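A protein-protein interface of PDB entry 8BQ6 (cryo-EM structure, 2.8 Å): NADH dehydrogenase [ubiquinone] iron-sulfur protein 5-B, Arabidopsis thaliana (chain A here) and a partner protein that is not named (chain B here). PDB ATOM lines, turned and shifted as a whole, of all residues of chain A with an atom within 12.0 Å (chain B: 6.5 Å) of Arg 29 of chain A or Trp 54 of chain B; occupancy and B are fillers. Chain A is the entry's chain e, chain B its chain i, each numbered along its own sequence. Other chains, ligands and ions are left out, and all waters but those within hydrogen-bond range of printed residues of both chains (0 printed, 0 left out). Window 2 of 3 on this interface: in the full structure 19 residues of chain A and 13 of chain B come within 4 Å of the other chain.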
ATOM      1  N   TRP A  18     -22.693   2.684 -29.512  1.00  0.00           N
ATOM      2  CA  TRP A  18     -21.418   2.909 -28.788  1.00  0.00           C
ATOM      3  C   TRP A  18     -21.467   2.189 -27.443  1.00  0.00           C
ATOM      4  O   TRP A  18     -20.498   1.507 -27.112  1.00  0.00           O
ATOM      5  CB  TRP A  18     -21.139   4.405 -28.589  1.00  0.00           C
ATOM      6  CG  TRP A  18     -20.031   4.622 -27.611  1.00  0.00           C
ATOM      7  CD1 TRP A  18     -20.125   5.112 -26.343  1.00  0.00           C
ATOM      8  CD2 TRP A  18     -18.654   4.266 -27.805  1.00  0.00           C
ATOM      9  NE1 TRP A  18     -18.897   5.111 -25.745  1.00  0.00           N
ATOM     10  CE2 TRP A  18     -17.975   4.599 -26.617  1.00  0.00           C
ATOM     11  CE3 TRP A  18     -17.932   3.715 -28.866  1.00  0.00           C
ATOM     12  CZ2 TRP A  18     -16.606   4.400 -26.467  1.00  0.00           C
ATOM     13  CZ3 TRP A  18     -16.583   3.513 -28.711  1.00  0.00           C
ATOM     14  CH2 TRP A  18     -15.929   3.854 -27.530  1.00  0.00           C
ATOM     15  N   MET A  19     -22.564   2.357 -26.705  1.00  0.00           N
ATOM     16  CA  MET A  19     -22.659   1.757 -25.381  1.00  0.00           C
ATOM     17  C   MET A  19     -22.666   0.235 -25.456  1.00  0.00           C
ATOM     18  O   MET A  19     -22.073  -0.430 -24.600  1.00  0.00           O
ATOM     19  CB  MET A  19     -23.896   2.274 -24.655  1.00  0.00           C
ATOM     20  CG  MET A  19     -23.727   3.681 -24.133  1.00  0.00           C
ATOM     21  SD  MET A  19     -22.062   3.945 -23.489  1.00  0.00           S
ATOM     22  CE  MET A  19     -22.412   4.283 -21.769  1.00  0.00           C
ATOM     23  N   ASP A  20     -23.323  -0.338 -26.468  1.00  0.00           N
ATOM     24  CA  ASP A  20     -23.250  -1.786 -26.658  1.00  0.00           C
ATOM     25  C   ASP A  20     -21.814  -2.235 -26.887  1.00  0.00           C
ATOM     26  O   ASP A  20     -21.341  -3.196 -26.264  1.00  0.00           O
ATOM     27  CB  ASP A  20     -24.125  -2.212 -27.833  1.00  0.00           C
ATOM     28  CG  ASP A  20     -25.585  -1.942 -27.595  1.00  0.00           C
ATOM     29  OD1 ASP A  20     -26.352  -1.930 -28.579  1.00  0.00           O
ATOM     30  OD2 ASP A  20     -25.970  -1.749 -26.424  1.00  0.00           O
ATOM     31  N   PHE A  21     -21.102  -1.541 -27.775  1.00  0.00           N
ATOM     32  CA  PHE A  21     -19.720  -1.912 -28.059  1.00  0.00           C
ATOM     33  C   PHE A  21     -18.844  -1.779 -26.816  1.00  0.00           C
ATOM     34  O   PHE A  21     -18.004  -2.645 -26.540  1.00  0.00           O
ATOM     35  CB  PHE A  21     -19.187  -1.051 -29.200  1.00  0.00           C
ATOM     36  CG  PHE A  21     -17.716  -1.183 -29.428  1.00  0.00           C
ATOM     37  CD1 PHE A  21     -17.164  -2.394 -29.783  1.00  0.00           C
ATOM     38  CD2 PHE A  21     -16.886  -0.086 -29.300  1.00  0.00           C
ATOM     39  CE1 PHE A  21     -15.810  -2.510 -29.999  1.00  0.00           C
ATOM     40  CE2 PHE A  21     -15.534  -0.197 -29.514  1.00  0.00           C
ATOM     41  CZ  PHE A  21     -14.996  -1.409 -29.866  1.00  0.00           C
ATOM     42  N   SER A  22     -19.038  -0.707 -26.047  1.00  0.00           N
ATOM     43  CA  SER A  22     -18.229  -0.490 -24.852  1.00  0.00           C
ATOM     44  C   SER A  22     -18.507  -1.548 -23.796  1.00  0.00           C
ATOM     45  O   SER A  22     -17.575  -2.088 -23.185  1.00  0.00           O
ATOM     46  CB  SER A  22     -18.494   0.902 -24.286  1.00  0.00           C
ATOM     47  OG  SER A  22     -18.062   1.898 -25.191  1.00  0.00           O
ATOM     48  N   GLU A  23     -19.782  -1.845 -23.552  1.00  0.00           N
ATOM     49  CA  GLU A  23     -20.118  -2.852 -22.557  1.00  0.00           C
ATOM     50  C   GLU A  23     -19.581  -4.218 -22.967  1.00  0.00           C
ATOM     51  O   GLU A  23     -19.087  -4.973 -22.122  1.00  0.00           O
ATOM     52  CB  GLU A  23     -21.632  -2.891 -22.338  1.00  0.00           C
ATOM     53  CG  GLU A  23     -22.198  -1.692 -21.617  1.00  0.00           C
ATOM     54  CD  GLU A  23     -23.680  -1.773 -21.381  1.00  0.00           C
ATOM     55  OE1 GLU A  23     -24.076  -2.373 -20.361  1.00  0.00           O
ATOM     56  OE2 GLU A  23     -24.453  -1.240 -22.204  1.00  0.00           O
ATOM     57  N   CYS A  24     -19.630  -4.543 -24.263  1.00  0.00           N
ATOM     58  CA  CYS A  24     -19.011  -5.787 -24.714  1.00  0.00           C
ATOM     59  C   CYS A  24     -17.509  -5.780 -24.453  1.00  0.00           C
ATOM     60  O   CYS A  24     -16.954  -6.763 -23.952  1.00  0.00           O
ATOM     61  CB  CYS A  24     -19.294  -6.026 -26.199  1.00  0.00           C
ATOM     62  SG  CYS A  24     -18.558  -7.553 -26.887  1.00  0.00           S
ATOM     63  N   MET A  25     -16.830  -4.675 -24.777  1.00  0.00           N
ATOM     64  CA  MET A  25     -15.378  -4.640 -24.616  1.00  0.00           C
ATOM     65  C   MET A  25     -14.937  -4.592 -23.159  1.00  0.00           C
ATOM     66  O   MET A  25     -13.764  -4.852 -22.874  1.00  0.00           O
ATOM     67  CB  MET A  25     -14.770  -3.444 -25.348  1.00  0.00           C
ATOM     68  CG  MET A  25     -14.787  -3.560 -26.851  1.00  0.00           C
ATOM     69  SD  MET A  25     -13.189  -4.002 -27.565  1.00  0.00           S
ATOM     70  CE  MET A  25     -12.108  -2.767 -26.853  1.00  0.00           C
ATOM     71  N   SER A  26     -15.831  -4.233 -22.240  1.00  0.00           N
ATOM     72  CA  SER A  26     -15.430  -4.131 -20.841  1.00  0.00           C
ATOM     73  C   SER A  26     -15.150  -5.481 -20.194  1.00  0.00           C
ATOM     74  O   SER A  26     -14.433  -5.527 -19.189  1.00  0.00           O
ATOM     75  CB  SER A  26     -16.502  -3.390 -20.045  1.00  0.00           C
ATOM     76  OG  SER A  26     -17.634  -4.213 -19.833  1.00  0.00           O
ATOM     77  N   HIS A  27     -15.689  -6.573 -20.730  1.00  0.00           N
ATOM     78  CA  HIS A  27     -15.446  -7.886 -20.146  1.00  0.00           C
ATOM     79  C   HIS A  27     -14.869  -8.894 -21.120  1.00  0.00           C
ATOM     80  O   HIS A  27     -14.294  -9.887 -20.669  1.00  0.00           O
ATOM     81  CB  HIS A  27     -16.743  -8.449 -19.555  1.00  0.00           C
ATOM     82  CG  HIS A  27     -17.870  -8.493 -20.533  1.00  0.00           C
ATOM     83  ND1 HIS A  27     -17.919  -9.394 -21.572  1.00  0.00           N
ATOM     84  CD2 HIS A  27     -18.973  -7.719 -20.653  1.00  0.00           C
ATOM     85  CE1 HIS A  27     -19.016  -9.190 -22.279  1.00  0.00           C
ATOM     86  NE2 HIS A  27     -19.673  -8.178 -21.743  1.00  0.00           N
ATOM     87  N   CYS A  28     -14.994  -8.687 -22.425  1.00  0.00           N
ATOM     88  CA  CYS A  28     -14.411  -9.590 -23.403  1.00  0.00           C
ATOM     89  C   CYS A  28     -12.918  -9.302 -23.497  1.00  0.00           C
ATOM     90  O   CYS A  28     -12.515  -8.211 -23.912  1.00  0.00           O
ATOM     91  CB  CYS A  28     -15.096  -9.426 -24.758  1.00  0.00           C
ATOM     92  SG  CYS A  28     -16.720 -10.214 -24.847  1.00  0.00           S
ATOM     93  N   ARG A  29     -12.082 -10.258 -23.099  1.00  0.00           N
ATOM     94  CA  ARG A  29     -10.616  -9.985 -23.076  1.00  0.00           C
ATOM     95  C   ARG A  29     -10.032  -9.989 -24.496  1.00  0.00           C
ATOM     96  O   ARG A  29      -8.837  -9.653 -24.624  1.00  0.00           O
ATOM     97  CB  ARG A  29      -9.903 -10.985 -22.159  1.00  0.00           C
ATOM     98  CG  ARG A  29     -10.471 -11.069 -20.750  1.00  0.00           C
ATOM     99  CD  ARG A  29      -9.537 -11.780 -19.787  1.00  0.00           C
ATOM    100  NE  ARG A  29      -8.842 -12.894 -20.419  1.00  0.00           N
ATOM    101  CZ  ARG A  29      -9.044 -14.177 -20.145  1.00  0.00           C
ATOM    102  NH1 ARG A  29      -9.925 -14.536 -19.228  1.00  0.00           N
ATOM    103  NH2 ARG A  29      -8.358 -15.101 -20.792  1.00  0.00           N
ATOM    104  N   GLU A  30     -10.822 -10.354 -25.516  1.00  0.00           N
ATOM    105  CA  GLU A  30     -10.348 -10.311 -26.895  1.00  0.00           C
ATOM    106  C   GLU A  30     -11.160  -9.303 -27.696  1.00  0.00           C
ATOM    107  O   GLU A  30     -12.396  -9.411 -27.745  1.00  0.00           O
ATOM    108  CB  GLU A  30     -10.435 -11.695 -27.547  1.00  0.00           C
ATOM    109  CG  GLU A  30      -9.380 -12.675 -27.067  1.00  0.00           C
ATOM    110  CD  GLU A  30      -9.962 -13.824 -26.270  1.00  0.00           C
ATOM    111  OE1 GLU A  30     -11.085 -14.268 -26.588  1.00  0.00           O
ATOM    112  OE2 GLU A  30      -9.296 -14.281 -25.319  1.00  0.00           O
ATOM    113  N   PRO A  31     -10.523  -8.331 -28.356  1.00  0.00           N
ATOM    114  CA  PRO A  31     -11.293  -7.360 -29.151  1.00  0.00           C
ATOM    115  C   PRO A  31     -12.094  -7.993 -30.273  1.00  0.00           C
ATOM    116  O   PRO A  31     -13.141  -7.451 -30.646  1.00  0.00           O
ATOM    117  CB  PRO A  31     -10.223  -6.403 -29.697  1.00  0.00           C
ATOM    118  CG  PRO A  31      -8.899  -7.027 -29.403  1.00  0.00           C
ATOM    119  CD  PRO A  31      -9.086  -8.310 -28.666  1.00  0.00           C
ATOM    120  N   LYS A  32     -11.644  -9.124 -30.817  1.00  0.00           N
ATOM    121  CA  LYS A  32     -12.369  -9.764 -31.906  1.00  0.00           C
ATOM    122  C   LYS A  32     -13.744 -10.259 -31.476  1.00  0.00           C
ATOM    123  O   LYS A  32     -14.615 -10.449 -32.332  1.00  0.00           O
ATOM    124  CB  LYS A  32     -11.547 -10.922 -32.465  1.00  0.00           C
ATOM    125  CG  LYS A  32     -10.423 -10.482 -33.376  1.00  0.00           C
ATOM    126  CD  LYS A  32      -9.555 -11.662 -33.773  1.00  0.00           C
ATOM    127  CE  LYS A  32      -8.544 -11.269 -34.832  1.00  0.00           C
ATOM    128  NZ  LYS A  32      -7.186 -11.081 -34.254  1.00  0.00           N
ATOM    129  N   ASP A  33     -13.963 -10.469 -30.179  1.00  0.00           N
ATOM    130  CA  ASP A  33     -15.278 -10.877 -29.707  1.00  0.00           C
ATOM    131  C   ASP A  33     -16.335  -9.798 -29.880  1.00  0.00           C
ATOM    132  O   ASP A  33     -17.527 -10.121 -29.917  1.00  0.00           O
ATOM    133  CB  ASP A  33     -15.220 -11.286 -28.235  1.00  0.00           C
ATOM    134  CG  ASP A  33     -14.314 -12.475 -27.991  1.00  0.00           C
ATOM    135  OD1 ASP A  33     -14.558 -13.211 -27.013  1.00  0.00           O
ATOM    136  OD2 ASP A  33     -13.356 -12.672 -28.767  1.00  0.00           O
ATOM    137  N   CYS A  34     -15.938  -8.529 -29.977  1.00  0.00           N
ATOM    138  CA  CYS A  34     -16.884  -7.428 -30.112  1.00  0.00           C
ATOM    139  C   CYS A  34     -16.811  -6.768 -31.486  1.00  0.00           C
ATOM    140  O   CYS A  34     -17.196  -5.605 -31.634  1.00  0.00           O
ATOM    141  CB  CYS A  34     -16.655  -6.394 -29.008  1.00  0.00           C
ATOM    142  SG  CYS A  34     -16.629  -7.076 -27.325  1.00  0.00           S
ATOM    143  N   THR A  35     -16.336  -7.501 -32.497  1.00  0.00           N
ATOM    144  CA  THR A  35     -16.164  -6.933 -33.832  1.00  0.00           C
ATOM    145  C   THR A  35     -17.496  -6.511 -34.446  1.00  0.00           C
ATOM    146  O   THR A  35     -17.592  -5.443 -35.068  1.00  0.00           O
ATOM    147  CB  THR A  35     -15.443  -7.952 -34.720  1.00  0.00           C
ATOM    148  OG1 THR A  35     -14.061  -8.008 -34.349  1.00  0.00           O
ATOM    149  CG2 THR A  35     -15.557  -7.594 -36.191  1.00  0.00           C
ATOM    150  N   LEU A  37     -20.345  -5.569 -32.992  1.00  0.00           N
ATOM    151  CA  LEU A  37     -20.839  -4.345 -32.367  1.00  0.00           C
ATOM    152  C   LEU A  37     -20.014  -3.134 -32.788  1.00  0.00           C
ATOM    153  O   LEU A  37     -20.555  -2.034 -32.979  1.00  0.00           O
ATOM    154  CB  LEU A  37     -20.834  -4.503 -30.848  1.00  0.00           C
ATOM    155  CG  LEU A  37     -21.551  -5.761 -30.360  1.00  0.00           C
ATOM    156  CD1 LEU A  37     -21.601  -5.807 -28.852  1.00  0.00           C
ATOM    157  CD2 LEU A  37     -22.948  -5.799 -30.935  1.00  0.00           C
ATOM    158  N   ARG A  38     -18.702  -3.317 -32.936  1.00  0.00           N
ATOM    159  CA  ARG A  38     -17.857  -2.214 -33.375  1.00  0.00           C
ATOM    160  C   ARG A  38     -18.243  -1.746 -34.770  1.00  0.00           C
ATOM    161  O   ARG A  38     -18.359  -0.537 -35.022  1.00  0.00           O
ATOM    162  CB  ARG A  38     -16.393  -2.631 -33.347  1.00  0.00           C
ATOM    163  CG  ARG A  38     -15.442  -1.521 -33.718  1.00  0.00           C
ATOM    164  CD  ARG A  38     -14.172  -2.104 -34.274  1.00  0.00           C
ATOM    165  NE  ARG A  38     -13.112  -1.115 -34.401  1.00  0.00           N
ATOM    166  CZ  ARG A  38     -12.616  -0.695 -35.555  1.00  0.00           C
ATOM    167  NH1 ARG A  38     -13.077  -1.145 -36.710  1.00  0.00           N
ATOM    168  NH2 ARG A  38     -11.631   0.198 -35.551  1.00  0.00           N
ATOM    169  N   ARG B  49       1.714  -3.818 -23.332  1.00  0.00           N
ATOM    170  CA  ARG B  49       0.263  -3.746 -23.382  1.00  0.00           C
ATOM    171  C   ARG B  49      -0.288  -5.045 -22.817  1.00  0.00           C
ATOM    172  O   ARG B  49      -0.179  -6.093 -23.471  1.00  0.00           O
ATOM    173  CB  ARG B  49      -0.206  -3.542 -24.824  1.00  0.00           C
ATOM    174  CG  ARG B  49      -1.707  -3.602 -25.008  1.00  0.00           C
ATOM    175  CD  ARG B  49      -2.094  -4.314 -26.299  1.00  0.00           C
ATOM    176  NE  ARG B  49      -1.227  -3.969 -27.421  1.00  0.00           N
ATOM    177  CZ  ARG B  49      -0.561  -4.852 -28.151  1.00  0.00           C
ATOM    178  NH1 ARG B  49      -0.627  -6.149 -27.899  1.00  0.00           N
ATOM    179  NH2 ARG B  49       0.188  -4.422 -29.164  1.00  0.00           N
ATOM    180  N   PRO B  50      -0.916  -5.107 -21.608  1.00  0.00           N
ATOM    181  CA  PRO B  50      -1.343  -6.417 -21.078  1.00  0.00           C
ATOM    182  C   PRO B  50      -2.550  -7.036 -21.803  1.00  0.00           C
ATOM    183  O   PRO B  50      -3.043  -6.462 -22.765  1.00  0.00           O
ATOM    184  CB  PRO B  50      -1.712  -6.128 -19.616  1.00  0.00           C
ATOM    185  CG  PRO B  50      -2.189  -4.700 -19.645  1.00  0.00           C
ATOM    186  CD  PRO B  50      -1.288  -4.025 -20.654  1.00  0.00           C
ATOM    187  N   TYR B  51      -3.005  -8.192 -21.317  1.00  0.00           N
ATOM    188  CA  TYR B  51      -4.140  -8.882 -21.974  1.00  0.00           C
ATOM    189  C   TYR B  51      -5.430  -8.137 -21.662  1.00  0.00           C
ATOM    190  O   TYR B  51      -5.982  -8.325 -20.556  1.00  0.00           O
ATOM    191  CB  TYR B  51      -4.273 -10.338 -21.530  1.00  0.00           C
ATOM    192  CG  TYR B  51      -4.930 -11.188 -22.586  1.00  0.00           C
ATOM    193  CD1 TYR B  51      -4.546 -11.071 -23.911  1.00  0.00           C
ATOM    194  CD2 TYR B  51      -5.948 -12.073 -22.276  1.00  0.00           C
ATOM    195  CE1 TYR B  51      -5.131 -11.840 -24.901  1.00  0.00           C
ATOM    196  CE2 TYR B  51      -6.542 -12.856 -23.254  1.00  0.00           C
ATOM    197  CZ  TYR B  51      -6.131 -12.735 -24.569  1.00  0.00           C
ATOM    198  OH  TYR B  51      -6.694 -13.492 -25.550  1.00  0.00           O
ATOM    199  N   GLY B  52      -5.887  -7.323 -22.614  1.00  0.00           N
ATOM    200  CA  GLY B  52      -7.139  -6.579 -22.422  1.00  0.00           C
ATOM    201  C   GLY B  52      -6.976  -5.465 -21.414  1.00  0.00           C
ATOM    202  O   GLY B  52      -7.526  -5.596 -20.316  1.00  0.00           O
ATOM    203  N   PHE B  53      -6.225  -4.415 -21.754  1.00  0.00           N
ATOM    204  CA  PHE B  53      -6.172  -3.267 -20.809  1.00  0.00           C
ATOM    205  C   PHE B  53      -7.601  -2.724 -20.698  1.00  0.00           C
ATOM    206  O   PHE B  53      -8.040  -2.532 -19.570  1.00  0.00           O
ATOM    207  CB  PHE B  53      -5.089  -2.252 -21.190  1.00  0.00           C
ATOM    208  CG  PHE B  53      -5.361  -1.361 -22.374  1.00  0.00           C
ATOM    209  CD1 PHE B  53      -4.910  -1.707 -23.634  1.00  0.00           C
ATOM    210  CD2 PHE B  53      -6.022  -0.151 -22.218  1.00  0.00           C
ATOM    211  CE1 PHE B  53      -5.143  -0.882 -24.721  1.00  0.00           C
ATOM    212  CE2 PHE B  53      -6.265   0.667 -23.308  1.00  0.00           C
ATOM    213  CZ  PHE B  53      -5.822   0.301 -24.556  1.00  0.00           C
ATOM    214  N   TRP B  54      -8.328  -2.621 -21.815  1.00  0.00           N
ATOM    215  CA  TRP B  54      -9.738  -2.132 -21.834  1.00  0.00           C
ATOM    216  C   TRP B  54     -10.572  -2.783 -20.718  1.00  0.00           C
ATOM    217  O   TRP B  54     -11.443  -2.083 -20.160  1.00  0.00           O
ATOM    218  CB  TRP B  54     -10.348  -2.341 -23.232  1.00  0.00           C
ATOM    219  CG  TRP B  54     -10.110  -3.682 -23.858  1.00  0.00           C
ATOM    220  CD1 TRP B  54     -10.917  -4.778 -23.780  1.00  0.00           C
ATOM    221  CD2 TRP B  54      -9.005  -4.066 -24.697  1.00  0.00           C
ATOM    222  NE1 TRP B  54     -10.393  -5.816 -24.498  1.00  0.00           N
ATOM    223  CE2 TRP B  54      -9.218  -5.410 -25.070  1.00  0.00           C
ATOM    224  CE3 TRP B  54      -7.857  -3.415 -25.158  1.00  0.00           C
ATOM    225  CZ2 TRP B  54      -8.322  -6.109 -25.875  1.00  0.00           C
ATOM    226  CZ3 TRP B  54      -6.973  -4.105 -25.954  1.00  0.00           C
ATOM    227  CH2 TRP B  54      -7.206  -5.433 -26.311  1.00  0.00           C
ATOM    228  N   THR B  55     -10.301  -4.051 -20.380  1.00  0.00           N
ATOM    229  CA  THR B  55     -11.050  -4.793 -19.325  1.00  0.00           C
ATOM    230  C   THR B  55     -10.922  -4.135 -17.938  1.00  0.00           C
ATOM    231  O   THR B  55     -11.885  -4.268 -17.166  1.00  0.00           O
ATOM    232  CB  THR B  55     -10.578  -6.257 -19.299  1.00  0.00           C
ATOM    233  OG1 THR B  55     -10.330  -6.699 -20.635  1.00  0.00           O
ATOM    234  CG2 THR B  55     -11.565  -7.205 -18.652  1.00  0.00           C
ATOM    235  N   PHE B  56      -9.827  -3.422 -17.629  1.00  0.00           N
ATOM    236  CA  PHE B  56      -9.581  -2.874 -16.257  1.00  0.00           C
ATOM    237  C   PHE B  56     -10.600  -1.805 -15.854  1.00  0.00           C
ATOM    238  O   PHE B  56     -11.103  -1.100 -16.752  1.00  0.00           O
ATOM    239  CB  PHE B  56      -8.168  -2.303 -16.127  1.00  0.00           C
ATOM    240  CG  PHE B  56      -7.043  -3.243 -16.478  1.00  0.00           C
ATOM    241  CD1 PHE B  56      -7.195  -4.619 -16.387  1.00  0.00           C
ATOM    242  CD2 PHE B  56      -5.816  -2.746 -16.886  1.00  0.00           C
ATOM    243  CE1 PHE B  56      -6.156  -5.474 -16.718  1.00  0.00           C
ATOM    244  CE2 PHE B  56      -4.775  -3.600 -17.211  1.00  0.00           C
ATOM    245  CZ  PHE B  56      -4.948  -4.962 -17.126  1.00  0.00           C
ATOM    246  N   GLU B  57     -10.822  -1.624 -14.544  1.00  0.00           N
ATOM    247  CA  GLU B  57     -11.870  -0.723 -14.072  1.00  0.00           C
ATOM    248  C   GLU B  57     -11.512   0.746 -14.265  1.00  0.00           C
ATOM    249  O   GLU B  57     -12.409   1.590 -14.363  1.00  0.00           O
ATOM    250  CB  GLU B  57     -12.167  -1.001 -12.598  1.00  0.00           C
ATOM    251  CG  GLU B  57     -13.584  -0.650 -12.173  1.00  0.00           C
ATOM    252  CD  GLU B  57     -13.654  -0.116 -10.754  1.00  0.00           C
ATOM    253  OE1 GLU B  57     -13.300   1.063 -10.547  1.00  0.00           O
ATOM    254  OE2 GLU B  57     -14.070  -0.869  -9.849  1.00  0.00           O
ATOM    255  N   HIS B  59     -10.380   1.862 -16.923  1.00  0.00           N
ATOM    256  CA  HIS B  59     -10.707   2.094 -18.321  1.00  0.00           C
ATOM    257  C   HIS B  59     -12.199   2.035 -18.611  1.00  0.00           C
ATOM    258  O   HIS B  59     -12.594   2.198 -19.769  1.00  0.00           O
ATOM    259  CB  HIS B  59      -9.983   1.067 -19.190  1.00  0.00           C
ATOM    260  CG  HIS B  59      -8.496   1.122 -19.059  1.00  0.00           C
ATOM    261  ND1 HIS B  59      -7.743   0.047 -18.640  1.00  0.00           N
ATOM    262  CD2 HIS B  59      -7.622   2.131 -19.273  1.00  0.00           C
ATOM    263  CE1 HIS B  59      -6.467   0.390 -18.611  1.00  0.00           C
ATOM    264  NE2 HIS B  59      -6.367   1.651 -18.993  1.00  0.00           N
ATOM    265  N   ASN B  60     -13.031   1.803 -17.599  1.00  0.00           N
ATOM    266  CA  ASN B  60     -14.479   1.734 -17.770  1.00  0.00           C
ATOM    267  C   ASN B  60     -15.192   2.840 -17.009  1.00  0.00           C
ATOM    268  O   ASN B  60     -16.230   2.611 -16.386  1.00  0.00           O
ATOM    269  CB  ASN B  60     -14.991   0.365 -17.338  1.00  0.00           C
ATOM    270  CG  ASN B  60     -14.329  -0.760 -18.098  1.00  0.00           C
ATOM    271  OD1 ASN B  60     -14.239  -0.723 -19.325  1.00  0.00           O
ATOM    272  ND2 ASN B  60     -13.834  -1.755 -17.372  1.00  0.00           N
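The backbone carbonyl oxygen (O) of Glu 23 of chain A lies within hydrogen-bond range of the side-chain hydroxyl (OG) of Ser 26 of chain A. The backbone carbonyl oxygen of Cys 24 of chain A sits close to the side-chain sulfur of Cys 28 of chain A (3.6 Å). SG of Cys 28 of chain A is in hydrogen-bond range of ND1 of His 27 of chain A. The backbone carbonyl oxygen (O) of Gly 52 of chain B is in hydrogen-bond range of the side-chain hydroxyl (OG1) of Thr 55 of chain B. The backbone carbonyl oxygen (O) of Trp 54 of chain B lies close to the side-chain amide oxygen (OD1) of Asn 60 of chain B (3.2 Å). SG of Cys 24 of chain A is disulfide-bonded to SG of Cys 34 of chain A, 2.0 Å away.
Met 25 of chain A touches Trp 54 of chain B. Ser 26 of chain A touches Asn 60 of chain B (CB to OD1, 3.6 Å). Arg 29 of chain A touches Tyr 51 of chain B. Arg 29 of chain A touches Trp 54 of chain B. Trp 54 of chain B touches Pro 31 of chain A (CZ2 to CD, 3.6 Å).
Of chain B, only Tyr 51 (3.5 Å) and Trp 54 (3.8 Å) come within 4 Å of Arg 29 of chain A. Of the printed residues of chain A, Trp 54 of chain B touches Met 25 (3.0 Å), Cys 28 (3.3 Å), Arg 29 (3.8 Å) and Pro 31 (3.6 Å). Pro 50 of chain B touches none of the printed residues of chain A. No residue of chain A comes within 4 Å of Gly 52 of chain B. No residue of chain A comes within 4 Å of Phe 53 of chain B. Thr 55 of chain B touches one residue of chain A. No residue of chain A comes within 4 Å of Phe 56 of chain B. Of chain A, only Ser 26 comes within 4 Å of Asn 60 of chain B. Printed residues of chain B within 4 Å of Ser 26 of chain A: Thr 55 (3.4 Å) and Asn 60 (3.6 Å). Printed residues of chain B within 4 Å of Cys 28 of chain A: Trp 54 (3.3 Å). His 27 of chain A touches none of the printed residues of chain B. Ser 22 of chain A touches none of the printed residues of chain B.
Of the 11 printed residues of chain B, 4 touch a printed residue of chain A. Along chain B the printed residues that touch a printed residue of chain A span positions 51 to 60. Printed residues of chain A that touch a printed residue of chain B: Met 25, Ser 26, Cys 28, Arg 29, Glu 30 and Pro 31. Hydrophobic or aromatic side chains of chain A that line the printed part of chain B: Met 25 and Pro 31. Among the printed residues, 8 pairs touch across the chains.
O of Cys 28 of chain A is in hydrogen-bond range of NE1 of Trp 54 of chain B, 3.3 Å away. OH of Tyr 51 of chain B is in hydrogen-bond range of OE2 of Glu 30 of chain A, at 2.7 Å. The backbone carbonyl oxygen of Ser 26 of chain A lies close to the backbone carbonyl oxygen of Thr 55 of chain B.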
